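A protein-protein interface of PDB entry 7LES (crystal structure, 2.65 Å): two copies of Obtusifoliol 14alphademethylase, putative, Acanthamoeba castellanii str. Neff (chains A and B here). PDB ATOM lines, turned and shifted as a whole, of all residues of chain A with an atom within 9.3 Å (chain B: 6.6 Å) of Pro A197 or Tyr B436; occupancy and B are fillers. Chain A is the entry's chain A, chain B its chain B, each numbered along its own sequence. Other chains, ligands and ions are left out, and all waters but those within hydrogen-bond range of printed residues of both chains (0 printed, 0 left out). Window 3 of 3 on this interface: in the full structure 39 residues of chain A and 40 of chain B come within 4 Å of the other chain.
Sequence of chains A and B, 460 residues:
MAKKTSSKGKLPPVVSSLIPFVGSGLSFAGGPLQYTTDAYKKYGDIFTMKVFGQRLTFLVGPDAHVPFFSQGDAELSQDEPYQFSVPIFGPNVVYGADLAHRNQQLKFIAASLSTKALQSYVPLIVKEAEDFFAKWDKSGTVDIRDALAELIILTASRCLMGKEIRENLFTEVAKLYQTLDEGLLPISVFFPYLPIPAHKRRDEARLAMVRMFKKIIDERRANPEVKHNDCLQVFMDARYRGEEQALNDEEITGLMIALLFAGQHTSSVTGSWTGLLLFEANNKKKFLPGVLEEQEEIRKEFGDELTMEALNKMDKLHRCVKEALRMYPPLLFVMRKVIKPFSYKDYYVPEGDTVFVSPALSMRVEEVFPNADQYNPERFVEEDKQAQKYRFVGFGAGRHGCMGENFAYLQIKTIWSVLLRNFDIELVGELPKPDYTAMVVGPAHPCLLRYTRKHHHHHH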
ATOM      1  N   THR A 179      28.617  -1.377 -11.081  1.00  0.00           N
ATOM      2  CA  THR A 179      28.202  -0.142 -11.756  1.00  0.00           C
ATOM      3  C   THR A 179      29.418   0.619 -12.298  1.00  0.00           C
ATOM      4  O   THR A 179      29.474   0.982 -13.477  1.00  0.00           O
ATOM      5  CB  THR A 179      27.420   0.803 -10.796  1.00  0.00           C
ATOM      6  OG1 THR A 179      26.448   0.060 -10.064  1.00  0.00           O
ATOM      7  CG2 THR A 179      26.684   1.876 -11.555  1.00  0.00           C
ATOM      8  N   GLU A 182      30.926  -0.966 -15.076  1.00  0.00           N
ATOM      9  CA  GLU A 182      29.991  -0.784 -16.195  1.00  0.00           C
ATOM     10  C   GLU A 182      29.966   0.609 -16.802  1.00  0.00           C
ATOM     11  O   GLU A 182      29.432   0.748 -17.898  1.00  0.00           O
ATOM     12  CB  GLU A 182      28.550  -1.123 -15.778  1.00  0.00           C
ATOM     13  CG  GLU A 182      28.218  -2.599 -15.725  1.00  0.00           C
ATOM     14  CD  GLU A 182      26.874  -2.897 -15.064  1.00  0.00           C
ATOM     15  OE1 GLU A 182      26.527  -4.104 -15.074  1.00  0.00           O
ATOM     16  OE2 GLU A 182      26.184  -1.961 -14.543  1.00  0.00           O
ATOM     17  N   GLY A 183      30.477   1.636 -16.100  1.00  0.00           N
ATOM     18  CA  GLY A 183      30.575   3.043 -16.633  1.00  0.00           C
ATOM     19  C   GLY A 183      31.918   3.392 -17.294  1.00  0.00           C
ATOM     20  O   GLY A 183      32.405   4.552 -17.299  1.00  0.00           O
ATOM     21  N   LEU A 184      32.534   2.356 -17.834  1.00  0.00           N
ATOM     22  CA  LEU A 184      33.820   2.464 -18.426  1.00  0.00           C
ATOM     23  C   LEU A 184      33.678   1.722 -19.732  1.00  0.00           C
ATOM     24  O   LEU A 184      33.922   0.510 -19.817  1.00  0.00           O
ATOM     25  CB  LEU A 184      34.881   1.880 -17.494  1.00  0.00           C
ATOM     26  CG  LEU A 184      36.317   1.877 -18.000  1.00  0.00           C
ATOM     27  CD1 LEU A 184      36.667   3.184 -18.692  1.00  0.00           C
ATOM     28  CD2 LEU A 184      37.240   1.619 -16.831  1.00  0.00           C
ATOM     29  N   LEU A 185      33.188   2.484 -20.711  1.00  0.00           N
ATOM     30  CA  LEU A 185      32.955   2.042 -22.067  1.00  0.00           C
ATOM     31  C   LEU A 185      34.065   2.634 -22.887  1.00  0.00           C
ATOM     32  O   LEU A 185      34.730   3.579 -22.423  1.00  0.00           O
ATOM     33  CB  LEU A 185      31.637   2.596 -22.585  1.00  0.00           C
ATOM     34  CG  LEU A 185      30.430   2.528 -21.652  1.00  0.00           C
ATOM     35  CD1 LEU A 185      29.227   3.204 -22.289  1.00  0.00           C
ATOM     36  CD2 LEU A 185      30.113   1.088 -21.318  1.00  0.00           C
ATOM     37  N   PRO A 186      34.250   2.124 -24.129  1.00  0.00           N
ATOM     38  CA  PRO A 186      35.251   2.711 -25.050  1.00  0.00           C
ATOM     39  C   PRO A 186      35.081   4.200 -25.213  1.00  0.00           C
ATOM     40  O   PRO A 186      36.064   4.913 -25.095  1.00  0.00           O
ATOM     41  CB  PRO A 186      35.007   1.978 -26.362  1.00  0.00           C
ATOM     42  CG  PRO A 186      34.469   0.660 -25.920  1.00  0.00           C
ATOM     43  CD  PRO A 186      33.620   0.925 -24.712  1.00  0.00           C
ATOM     44  N   ILE A 187      33.845   4.664 -25.411  1.00  0.00           N
ATOM     45  CA  ILE A 187      33.544   6.114 -25.386  1.00  0.00           C
ATOM     46  C   ILE A 187      34.088   6.836 -24.137  1.00  0.00           C
ATOM     47  O   ILE A 187      34.522   7.977 -24.244  1.00  0.00           O
ATOM     48  CB  ILE A 187      32.019   6.390 -25.570  1.00  0.00           C
ATOM     49  CG1 ILE A 187      31.721   7.867 -25.837  1.00  0.00           C
ATOM     50  CG2 ILE A 187      31.189   5.885 -24.405  1.00  0.00           C
ATOM     51  CD1 ILE A 187      32.175   8.317 -27.206  1.00  0.00           C
ATOM     52  N   SER A 188      34.097   6.169 -22.976  1.00  0.00           N
ATOM     53  CA  SER A 188      34.569   6.774 -21.715  1.00  0.00           C
ATOM     54  C   SER A 188      36.067   7.151 -21.612  1.00  0.00           C
ATOM     55  O   SER A 188      36.445   7.939 -20.702  1.00  0.00           O
ATOM     56  CB  SER A 188      34.216   5.883 -20.526  1.00  0.00           C
ATOM     57  OG  SER A 188      32.924   5.352 -20.664  1.00  0.00           O
ATOM     58  N   LEU A 194      30.757  12.771 -20.723  1.00  0.00           N
ATOM     59  CA  LEU A 194      29.624  12.730 -21.630  1.00  0.00           C
ATOM     60  C   LEU A 194      28.384  12.260 -20.870  1.00  0.00           C
ATOM     61  O   LEU A 194      28.407  11.181 -20.281  1.00  0.00           O
ATOM     62  CB  LEU A 194      29.916  11.736 -22.740  1.00  0.00           C
ATOM     63  CG  LEU A 194      28.881  11.573 -23.839  1.00  0.00           C
ATOM     64  CD1 LEU A 194      28.907  12.819 -24.701  1.00  0.00           C
ATOM     65  CD2 LEU A 194      29.174  10.334 -24.672  1.00  0.00           C
ATOM     66  N   PRO A 195      27.300  13.053 -20.880  1.00  0.00           N
ATOM     67  CA  PRO A 195      26.110  12.655 -20.147  1.00  0.00           C
ATOM     68  C   PRO A 195      25.307  11.601 -20.908  1.00  0.00           C
ATOM     69  O   PRO A 195      24.454  11.916 -21.739  1.00  0.00           O
ATOM     70  CB  PRO A 195      25.344  13.967 -19.983  1.00  0.00           C
ATOM     71  CG  PRO A 195      25.703  14.744 -21.189  1.00  0.00           C
ATOM     72  CD  PRO A 195      27.096  14.323 -21.594  1.00  0.00           C
ATOM     73  N   ILE A 196      25.623  10.350 -20.604  1.00  0.00           N
ATOM     74  CA  ILE A 196      24.946   9.173 -21.140  1.00  0.00           C
ATOM     75  C   ILE A 196      24.520   8.333 -19.950  1.00  0.00           C
ATOM     76  O   ILE A 196      25.129   8.439 -18.882  1.00  0.00           O
ATOM     77  CB  ILE A 196      25.870   8.340 -22.056  1.00  0.00           C
ATOM     78  CG1 ILE A 196      27.273   8.125 -21.443  1.00  0.00           C
ATOM     79  CG2 ILE A 196      26.015   9.031 -23.396  1.00  0.00           C
ATOM     80  CD1 ILE A 196      28.054   6.967 -22.040  1.00  0.00           C
ATOM     81  N   PRO A 197      23.489   7.484 -20.102  1.00  0.00           N
ATOM     82  CA  PRO A 197      23.041   6.851 -18.848  1.00  0.00           C
ATOM     83  C   PRO A 197      24.159   6.180 -18.034  1.00  0.00           C
ATOM     84  O   PRO A 197      24.182   6.317 -16.819  1.00  0.00           O
ATOM     85  CB  PRO A 197      21.970   5.852 -19.316  1.00  0.00           C
ATOM     86  CG  PRO A 197      21.420   6.472 -20.558  1.00  0.00           C
ATOM     87  CD  PRO A 197      22.541   7.250 -21.209  1.00  0.00           C
ATOM     88  N   ALA A 198      25.097   5.517 -18.705  1.00  0.00           N
ATOM     89  CA  ALA A 198      26.152   4.763 -18.026  1.00  0.00           C
ATOM     90  C   ALA A 198      27.014   5.618 -17.120  1.00  0.00           C
ATOM     91  O   ALA A 198      27.458   5.128 -16.084  1.00  0.00           O
ATOM     92  CB  ALA A 198      27.030   4.043 -19.034  1.00  0.00           C
ATOM     93  N   HIS A 199      27.251   6.872 -17.501  1.00  0.00           N
ATOM     94  CA  HIS A 199      28.038   7.795 -16.676  1.00  0.00           C
ATOM     95  C   HIS A 199      27.217   8.437 -15.566  1.00  0.00           C
ATOM     96  O   HIS A 199      27.776   8.746 -14.519  1.00  0.00           O
ATOM     97  CB  HIS A 199      28.702   8.887 -17.516  1.00  0.00           C
ATOM     98  CG  HIS A 199      29.749   8.376 -18.449  1.00  0.00           C
ATOM     99  ND1 HIS A 199      30.318   9.159 -19.425  1.00  0.00           N
ATOM    100  CD2 HIS A 199      30.325   7.156 -18.569  1.00  0.00           C
ATOM    101  CE1 HIS A 199      31.210   8.451 -20.099  1.00  0.00           C
ATOM    102  NE2 HIS A 199      31.238   7.234 -19.596  1.00  0.00           N
ATOM    103  N   LYS A 200      25.918   8.659 -15.796  1.00  0.00           N
ATOM    104  CA  LYS A 200      25.011   9.112 -14.743  1.00  0.00           C
ATOM    105  C   LYS A 200      24.943   8.039 -13.641  1.00  0.00           C
ATOM    106  O   LYS A 200      25.054   8.359 -12.464  1.00  0.00           O
ATOM    107  CB  LYS A 200      23.616   9.438 -15.312  1.00  0.00           C
ATOM    108  CG  LYS A 200      22.639  10.102 -14.339  1.00  0.00           C
ATOM    109  N   ARG A 201      24.805   6.767 -14.016  1.00  0.00           N
ATOM    110  CA  ARG A 201      24.784   5.647 -13.039  1.00  0.00           C
ATOM    111  C   ARG A 201      26.123   5.468 -12.263  1.00  0.00           C
ATOM    112  O   ARG A 201      26.138   5.088 -11.097  1.00  0.00           O
ATOM    113  CB  ARG A 201      24.377   4.327 -13.728  1.00  0.00           C
ATOM    114  CG  ARG A 201      22.888   4.200 -14.005  1.00  0.00           C
ATOM    115  CD  ARG A 201      22.463   2.778 -14.357  1.00  0.00           C
ATOM    116  NE  ARG A 201      22.711   2.491 -15.776  1.00  0.00           N
ATOM    117  CZ  ARG A 201      23.582   1.598 -16.273  1.00  0.00           C
ATOM    118  NH1 ARG A 201      23.686   1.474 -17.598  1.00  0.00           N
ATOM    119  NH2 ARG A 201      24.344   0.818 -15.491  1.00  0.00           N
ATOM    120  N   ARG A 202      27.233   5.736 -12.939  1.00  0.00           N
ATOM    121  CA  ARG A 202      28.573   5.657 -12.362  1.00  0.00           C
ATOM    122  C   ARG A 202      28.750   6.697 -11.298  1.00  0.00           C
ATOM    123  O   ARG A 202      29.149   6.365 -10.178  1.00  0.00           O
ATOM    124  CB  ARG A 202      29.616   5.901 -13.460  1.00  0.00           C
ATOM    125  CG  ARG A 202      31.075   5.988 -13.026  1.00  0.00           C
ATOM    126  CD  ARG A 202      31.875   6.647 -14.121  1.00  0.00           C
ATOM    127  NE  ARG A 202      31.448   8.029 -14.327  1.00  0.00           N
ATOM    128  CZ  ARG A 202      31.815   8.780 -15.360  1.00  0.00           C
ATOM    129  NH1 ARG A 202      32.627   8.294 -16.311  1.00  0.00           N
ATOM    130  NH2 ARG A 202      31.380  10.031 -15.444  1.00  0.00           N
ATOM    131  N   ASP A 203      28.470   7.948 -11.660  1.00  0.00           N
ATOM    132  CA  ASP A 203      28.585   9.066 -10.727  1.00  0.00           C
ATOM    133  C   ASP A 203      27.696   8.851  -9.503  1.00  0.00           C
ATOM    134  O   ASP A 203      28.137   9.058  -8.374  1.00  0.00           O
ATOM    135  CB  ASP A 203      28.236  10.394 -11.392  1.00  0.00           C
ATOM    136  CG  ASP A 203      29.209  10.783 -12.511  1.00  0.00           C
ATOM    137  OD1 ASP A 203      30.337  10.224 -12.556  1.00  0.00           O
ATOM    138  OD2 ASP A 203      28.825  11.654 -13.349  1.00  0.00           O
ATOM    139  N   GLU A 204      26.467   8.391  -9.713  1.00  0.00           N
ATOM    140  CA  GLU A 204      25.599   8.056  -8.571  1.00  0.00           C
ATOM    141  C   GLU A 204      26.245   6.968  -7.678  1.00  0.00           C
ATOM    142  O   GLU A 204      26.260   7.111  -6.471  1.00  0.00           O
ATOM    143  CB  GLU A 204      24.146   7.731  -9.007  1.00  0.00           C
ATOM    144  CG  GLU A 204      23.299   8.996  -9.256  1.00  0.00           C
ATOM    145  CD  GLU A 204      22.070   8.793 -10.151  1.00  0.00           C
ATOM    146  OE1 GLU A 204      21.504   9.807 -10.638  1.00  0.00           O
ATOM    147  OE2 GLU A 204      21.657   7.633 -10.378  1.00  0.00           O
ATOM    148  N   ALA A 205      26.835   5.934  -8.255  1.00  0.00           N
ATOM    149  CA  ALA A 205      27.419   4.858  -7.449  1.00  0.00           C
ATOM    150  C   ALA A 205      28.676   5.315  -6.701  1.00  0.00           C
ATOM    151  O   ALA A 205      28.936   4.867  -5.576  1.00  0.00           O
ATOM    152  CB  ALA A 205      27.710   3.626  -8.304  1.00  0.00           C
ATOM    153  N   SER B  27      27.136   5.435 -33.156  1.00  0.00           N
ATOM    154  CA  SER B  27      26.454   4.167 -32.910  1.00  0.00           C
ATOM    155  C   SER B  27      26.977   3.454 -31.635  1.00  0.00           C
ATOM    156  O   SER B  27      26.228   2.679 -31.038  1.00  0.00           O
ATOM    157  CB  SER B  27      26.547   3.268 -34.154  1.00  0.00           C
ATOM    158  OG  SER B  27      25.895   3.856 -35.287  1.00  0.00           O
ATOM    159  N   PHE B  28      28.235   3.751 -31.250  1.00  0.00           N
ATOM    160  CA  PHE B  28      28.925   3.260 -30.042  1.00  0.00           C
ATOM    161  C   PHE B  28      29.370   4.375 -29.100  1.00  0.00           C
ATOM    162  O   PHE B  28      30.411   4.263 -28.481  1.00  0.00           O
ATOM    163  CB  PHE B  28      30.188   2.494 -30.448  1.00  0.00           C
ATOM    164  CG  PHE B  28      29.906   1.203 -31.127  1.00  0.00           C
ATOM    165  CD1 PHE B  28      29.691   1.162 -32.495  1.00  0.00           C
ATOM    166  CD2 PHE B  28      29.842   0.006 -30.399  1.00  0.00           C
ATOM    167  CE1 PHE B  28      29.429  -0.047 -33.130  1.00  0.00           C
ATOM    168  CE2 PHE B  28      29.580  -1.211 -31.027  1.00  0.00           C
ATOM    169  CZ  PHE B  28      29.372  -1.238 -32.399  1.00  0.00           C
ATOM    170  N   ALA B  29      28.606   5.452 -28.970  1.00  0.00           N
ATOM    171  CA  ALA B  29      28.928   6.491 -27.968  1.00  0.00           C
ATOM    172  C   ALA B  29      28.098   6.329 -26.694  1.00  0.00           C
ATOM    173  O   ALA B  29      28.051   7.233 -25.859  1.00  0.00           O
ATOM    174  CB  ALA B  29      28.725   7.880 -28.560  1.00  0.00           C
ATOM    175  N   GLY B  30      27.422   5.189 -26.556  1.00  0.00           N
ATOM    176  CA  GLY B  30      26.719   4.870 -25.332  1.00  0.00           C
ATOM    177  C   GLY B  30      25.443   5.657 -25.136  1.00  0.00           C
ATOM    178  O   GLY B  30      25.002   5.819 -23.998  1.00  0.00           O
ATOM    179  N   GLY B  31      24.843   6.128 -26.237  1.00  0.00           N
ATOM    180  CA  GLY B  31      23.511   6.758 -26.203  1.00  0.00           C
ATOM    181  C   GLY B  31      23.448   8.204 -25.721  1.00  0.00           C
ATOM    182  O   GLY B  31      22.741   8.521 -24.747  1.00  0.00           O
ATOM    183  N   PRO B  32      24.134   9.116 -26.431  1.00  0.00           N
ATOM    184  CA  PRO B  32      24.088  10.531 -26.090  1.00  0.00           C
ATOM    185  C   PRO B  32      22.787  11.210 -26.516  1.00  0.00           C
ATOM    186  O   PRO B  32      22.823  12.335 -26.998  1.00  0.00           O
ATOM    187  CB  PRO B  32      25.281  11.094 -26.877  1.00  0.00           C
ATOM    188  CG  PRO B  32      25.328  10.260 -28.102  1.00  0.00           C
ATOM    189  CD  PRO B  32      24.948   8.876 -27.642  1.00  0.00           C
ATOM    190  N   LEU B  33      21.644  10.552 -26.321  1.00  0.00           N
ATOM    191  CA  LEU B  33      20.352  11.109 -26.717  1.00  0.00           C
ATOM    192  C   LEU B  33      20.065  12.295 -25.825  1.00  0.00           C
ATOM    193  O   LEU B  33      19.500  13.299 -26.269  1.00  0.00           O
ATOM    194  CB  LEU B  33      19.238  10.082 -26.556  1.00  0.00           C
ATOM    195  CG  LEU B  33      19.363   8.818 -27.401  1.00  0.00           C
ATOM    196  CD1 LEU B  33      18.276   7.806 -27.033  1.00  0.00           C
ATOM    197  CD2 LEU B  33      19.330   9.173 -28.879  1.00  0.00           C
ATOM    198  N   GLN B  34      20.474  12.168 -24.565  1.00  0.00           N
ATOM    199  CA  GLN B  34      20.457  13.282 -23.646  1.00  0.00           C
ATOM    200  C   GLN B  34      21.190  14.520 -24.213  1.00  0.00           C
ATOM    201  O   GLN B  34      20.541  15.529 -24.450  1.00  0.00           O
ATOM    202  CB  GLN B  34      21.022  12.848 -22.275  1.00  0.00           C
ATOM    203  CG  GLN B  34      20.898  13.879 -21.154  1.00  0.00           C
ATOM    204  CD  GLN B  34      19.600  14.682 -21.212  1.00  0.00           C
ATOM    205  OE1 GLN B  34      18.500  14.121 -21.280  1.00  0.00           O
ATOM    206  NE2 GLN B  34      19.726  16.003 -21.205  1.00  0.00           N
ATOM    207  N   TYR B 328      11.343   3.750 -28.867  1.00  0.00           N
ATOM    208  CA  TYR B 328      12.651   3.132 -28.721  1.00  0.00           C
ATOM    209  C   TYR B 328      13.114   2.575 -30.050  1.00  0.00           C
ATOM    210  O   TYR B 328      13.188   1.362 -30.221  1.00  0.00           O
ATOM    211  CB  TYR B 328      12.603   2.053 -27.629  1.00  0.00           C
ATOM    212  CG  TYR B 328      12.131   2.630 -26.320  1.00  0.00           C
ATOM    213  CD1 TYR B 328      12.919   3.554 -25.630  1.00  0.00           C
ATOM    214  CD2 TYR B 328      10.884   2.295 -25.796  1.00  0.00           C
ATOM    215  CE1 TYR B 328      12.481   4.123 -24.441  1.00  0.00           C
ATOM    216  CE2 TYR B 328      10.440   2.848 -24.607  1.00  0.00           C
ATOM    217  CZ  TYR B 328      11.234   3.766 -23.932  1.00  0.00           C
ATOM    218  OH  TYR B 328      10.785   4.328 -22.765  1.00  0.00           O
ATOM    219  N   LEU B 332      19.603   4.331 -33.979  1.00  0.00           N
ATOM    220  CA  LEU B 332      19.508   5.660 -33.338  1.00  0.00           C
ATOM    221  C   LEU B 332      19.926   6.778 -34.264  1.00  0.00           C
ATOM    222  O   LEU B 332      19.440   7.884 -34.111  1.00  0.00           O
ATOM    223  CB  LEU B 332      20.425   5.737 -32.096  1.00  0.00           C
ATOM    224  CG  LEU B 332      19.928   5.479 -30.667  1.00  0.00           C
ATOM    225  CD1 LEU B 332      18.875   4.391 -30.561  1.00  0.00           C
ATOM    226  CD2 LEU B 332      21.123   5.133 -29.800  1.00  0.00           C
ATOM    227  N   LYS B 433      14.957  -0.048 -19.135  1.00  0.00           N
ATOM    228  CA  LYS B 433      15.556   1.119 -19.788  1.00  0.00           C
ATOM    229  C   LYS B 433      16.397   0.541 -20.942  1.00  0.00           C
ATOM    230  O   LYS B 433      16.795  -0.619 -20.888  1.00  0.00           O
ATOM    231  CB  LYS B 433      16.425   1.959 -18.829  1.00  0.00           C
ATOM    232  CG  LYS B 433      15.880   2.149 -17.405  1.00  0.00           C
ATOM    233  CD  LYS B 433      15.620   3.601 -16.988  1.00  0.00           C
ATOM    234  CE  LYS B 433      14.291   4.134 -17.505  1.00  0.00           C
ATOM    235  NZ  LYS B 433      13.089   3.461 -16.921  1.00  0.00           N
ATOM    236  N   PRO B 434      16.641   1.328 -22.000  1.00  0.00           N
ATOM    237  CA  PRO B 434      17.346   0.765 -23.141  1.00  0.00           C
ATOM    238  C   PRO B 434      18.806   0.486 -22.834  1.00  0.00           C
ATOM    239  O   PRO B 434      19.406   1.213 -22.067  1.00  0.00           O
ATOM    240  CB  PRO B 434      17.242   1.865 -24.206  1.00  0.00           C
ATOM    241  CG  PRO B 434      16.154   2.773 -23.751  1.00  0.00           C
ATOM    242  CD  PRO B 434      16.179   2.699 -22.262  1.00  0.00           C
ATOM    243  N   ASP B 435      19.352  -0.559 -23.447  1.00  0.00           N
ATOM    244  CA  ASP B 435      20.760  -0.907 -23.339  1.00  0.00           C
ATOM    245  C   ASP B 435      21.507  -0.283 -24.501  1.00  0.00           C
ATOM    246  O   ASP B 435      21.372  -0.745 -25.622  1.00  0.00           O
ATOM    247  CB  ASP B 435      20.930  -2.434 -23.394  1.00  0.00           C
ATOM    248  CG  ASP B 435      22.392  -2.870 -23.502  1.00  0.00           C
ATOM    249  OD1 ASP B 435      23.303  -2.116 -23.090  1.00  0.00           O
ATOM    250  OD2 ASP B 435      22.624  -3.983 -23.994  1.00  0.00           O
ATOM    251  N   TYR B 436      22.339   0.721 -24.218  1.00  0.00           N
ATOM    252  CA  TYR B 436      23.141   1.427 -25.249  1.00  0.00           C
ATOM    253  C   TYR B 436      24.569   0.872 -25.514  1.00  0.00           C
ATOM    254  O   TYR B 436      25.344   1.510 -26.202  1.00  0.00           O
ATOM    255  CB  TYR B 436      23.207   2.924 -24.907  1.00  0.00           C
ATOM    256  CG  TYR B 436      21.853   3.621 -24.796  1.00  0.00           C
ATOM    257  CD1 TYR B 436      21.164   4.057 -25.938  1.00  0.00           C
ATOM    258  CD2 TYR B 436      21.265   3.863 -23.554  1.00  0.00           C
ATOM    259  CE1 TYR B 436      19.932   4.701 -25.843  1.00  0.00           C
ATOM    260  CE2 TYR B 436      20.030   4.514 -23.459  1.00  0.00           C
ATOM    261  CZ  TYR B 436      19.376   4.929 -24.607  1.00  0.00           C
ATOM    262  OH  TYR B 436      18.169   5.568 -24.510  1.00  0.00           O
ATOM    263  N   THR B 437      24.904  -0.304 -24.995  1.00  0.00           N
ATOM    264  CA  THR B 437      26.155  -1.010 -25.338  1.00  0.00           C
ATOM    265  C   THR B 437      26.345  -1.360 -26.819  1.00  0.00           C
ATOM    266  O   THR B 437      27.380  -1.055 -27.399  1.00  0.00           O
ATOM    267  CB  THR B 437      26.225  -2.357 -24.588  1.00  0.00           C
ATOM    268  OG1 THR B 437      26.060  -2.101 -23.197  1.00  0.00           O
ATOM    269  CG2 THR B 437      27.570  -3.124 -24.846  1.00  0.00           C
ATOM    270  N   ALA B 438      25.378  -2.061 -27.400  1.00  0.00           N
ATOM    271  CA  ALA B 438      25.525  -2.583 -28.762  1.00  0.00           C
ATOM    272  C   ALA B 438      25.130  -1.533 -29.806  1.00  0.00           C
ATOM    273  O   ALA B 438      24.593  -0.471 -29.487  1.00  0.00           O
ATOM    274  CB  ALA B 438      24.713  -3.863 -28.941  1.00  0.00           C
ATOM    275  N   MET B 439      25.409  -1.844 -31.060  1.00  0.00           N
ATOM    276  CA  MET B 439      25.047  -0.964 -32.167  1.00  0.00           C
ATOM    277  C   MET B 439      23.531  -0.878 -32.329  1.00  0.00           C
ATOM    278  O   MET B 439      23.001   0.176 -32.640  1.00  0.00           O
ATOM    279  CB  MET B 439      25.674  -1.455 -33.480  1.00  0.00           C
ATOM    280  CG  MET B 439      26.022  -0.337 -34.437  1.00  0.00           C
ATOM    281  SD  MET B 439      26.462  -0.887 -36.097  1.00  0.00           S
ATOM    282  CE  MET B 439      28.057  -1.644 -35.862  1.00  0.00           C
ATOM    283  N   VAL B 440      22.843  -1.998 -32.140  1.00  0.00           N
ATOM    284  CA  VAL B 440      21.390  -2.016 -32.164  1.00  0.00           C
ATOM    285  C   VAL B 440      20.928  -1.889 -30.717  1.00  0.00           C
ATOM    286  O   VAL B 440      21.318  -2.709 -29.878  1.00  0.00           O
ATOM    287  CB  VAL B 440      20.852  -3.315 -32.808  1.00  0.00           C
ATOM    288  CG1 VAL B 440      19.328  -3.358 -32.748  1.00  0.00           C
ATOM    289  CG2 VAL B 440      21.321  -3.430 -34.252  1.00  0.00           C
ATOM    290  N   VAL B 441      20.122  -0.864 -30.426  1.00  0.00           N
ATOM    291  CA  VAL B 441      19.632  -0.616 -29.060  1.00  0.00           C
ATOM    292  C   VAL B 441      18.365  -1.393 -28.806  1.00  0.00           C
ATOM    293  O   VAL B 441      17.373  -1.221 -29.518  1.00  0.00           O
ATOM    294  CB  VAL B 441      19.339   0.878 -28.797  1.00  0.00           C
ATOM    295  CG1 VAL B 441      18.679   1.094 -27.425  1.00  0.00           C
ATOM    296  CG2 VAL B 441      20.626   1.677 -28.917  1.00  0.00           C
ATOM    297  N   GLY B 442      18.404  -2.220 -27.768  1.00  0.00           N
ATOM    298  CA  GLY B 442      17.221  -2.932 -27.279  1.00  0.00           C
ATOM    299  C   GLY B 442      16.958  -2.666 -25.806  1.00  0.00           C
ATOM    300  O   GLY B 442      17.741  -1.971 -25.149  1.00  0.00           O
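Printed residues of chain B within 4 Å of Pro A197: Gly B30, Gly B31 and Tyr B436. Of chain A, only Pro A197 comes within 4 Å of Tyr B436. No residue of chain A comes within 4 Å of Pro B434. No residue of chain A comes within 4 Å of Thr B437. Of the printed residues of chain A, Phe B28 touches Ile A187 (3.9 Å). Printed residues of chain A within 4 Å of Gln B34: Pro A195 (3.6 Å). Of the printed residues of chain A, Ala B29 touches Ile A187 (3.7 Å), Leu A194 (3.5 Å) and Ile A196 (3.7 Å). Printed residues of chain A within 4 Å of Pro B32: Ile A196. The nearest printed residue of chain B that does not touch Leu A194 is Pro B32 (4.5 Å).
O of Leu A194 lies within hydrogen-bond range of ND1 of His A199.
No position is printed for both chains. Of the 11 pairs that touch across the chains among the printed residues, none has its exchanged pair printed and touching as well.
Hydrophobic or aromatic side chains of chain A that line the printed part of chain B: Ile A187, Leu A194, Ile A196 and Pro A197. Among the printed residues, no Asp or Glu carboxylate lies within 4 Å of a Lys or Arg side-chain nitrogen of the other chain.
Among the printed residues, merely in contact across the chains: Ile A187 with Phe B28, Ile A187 with Ala B29, Leu A194 with Ala B29, Pro A195 with Gln B34, Ile A196 with Ala B29, Ile A196 with Gly B30, Ile A196 with Gly B31, Ile A196 with Pro B32, Pro A197 with Gly B30, Pro A197 with Gly B31 and Pro A197 with Tyr B436.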
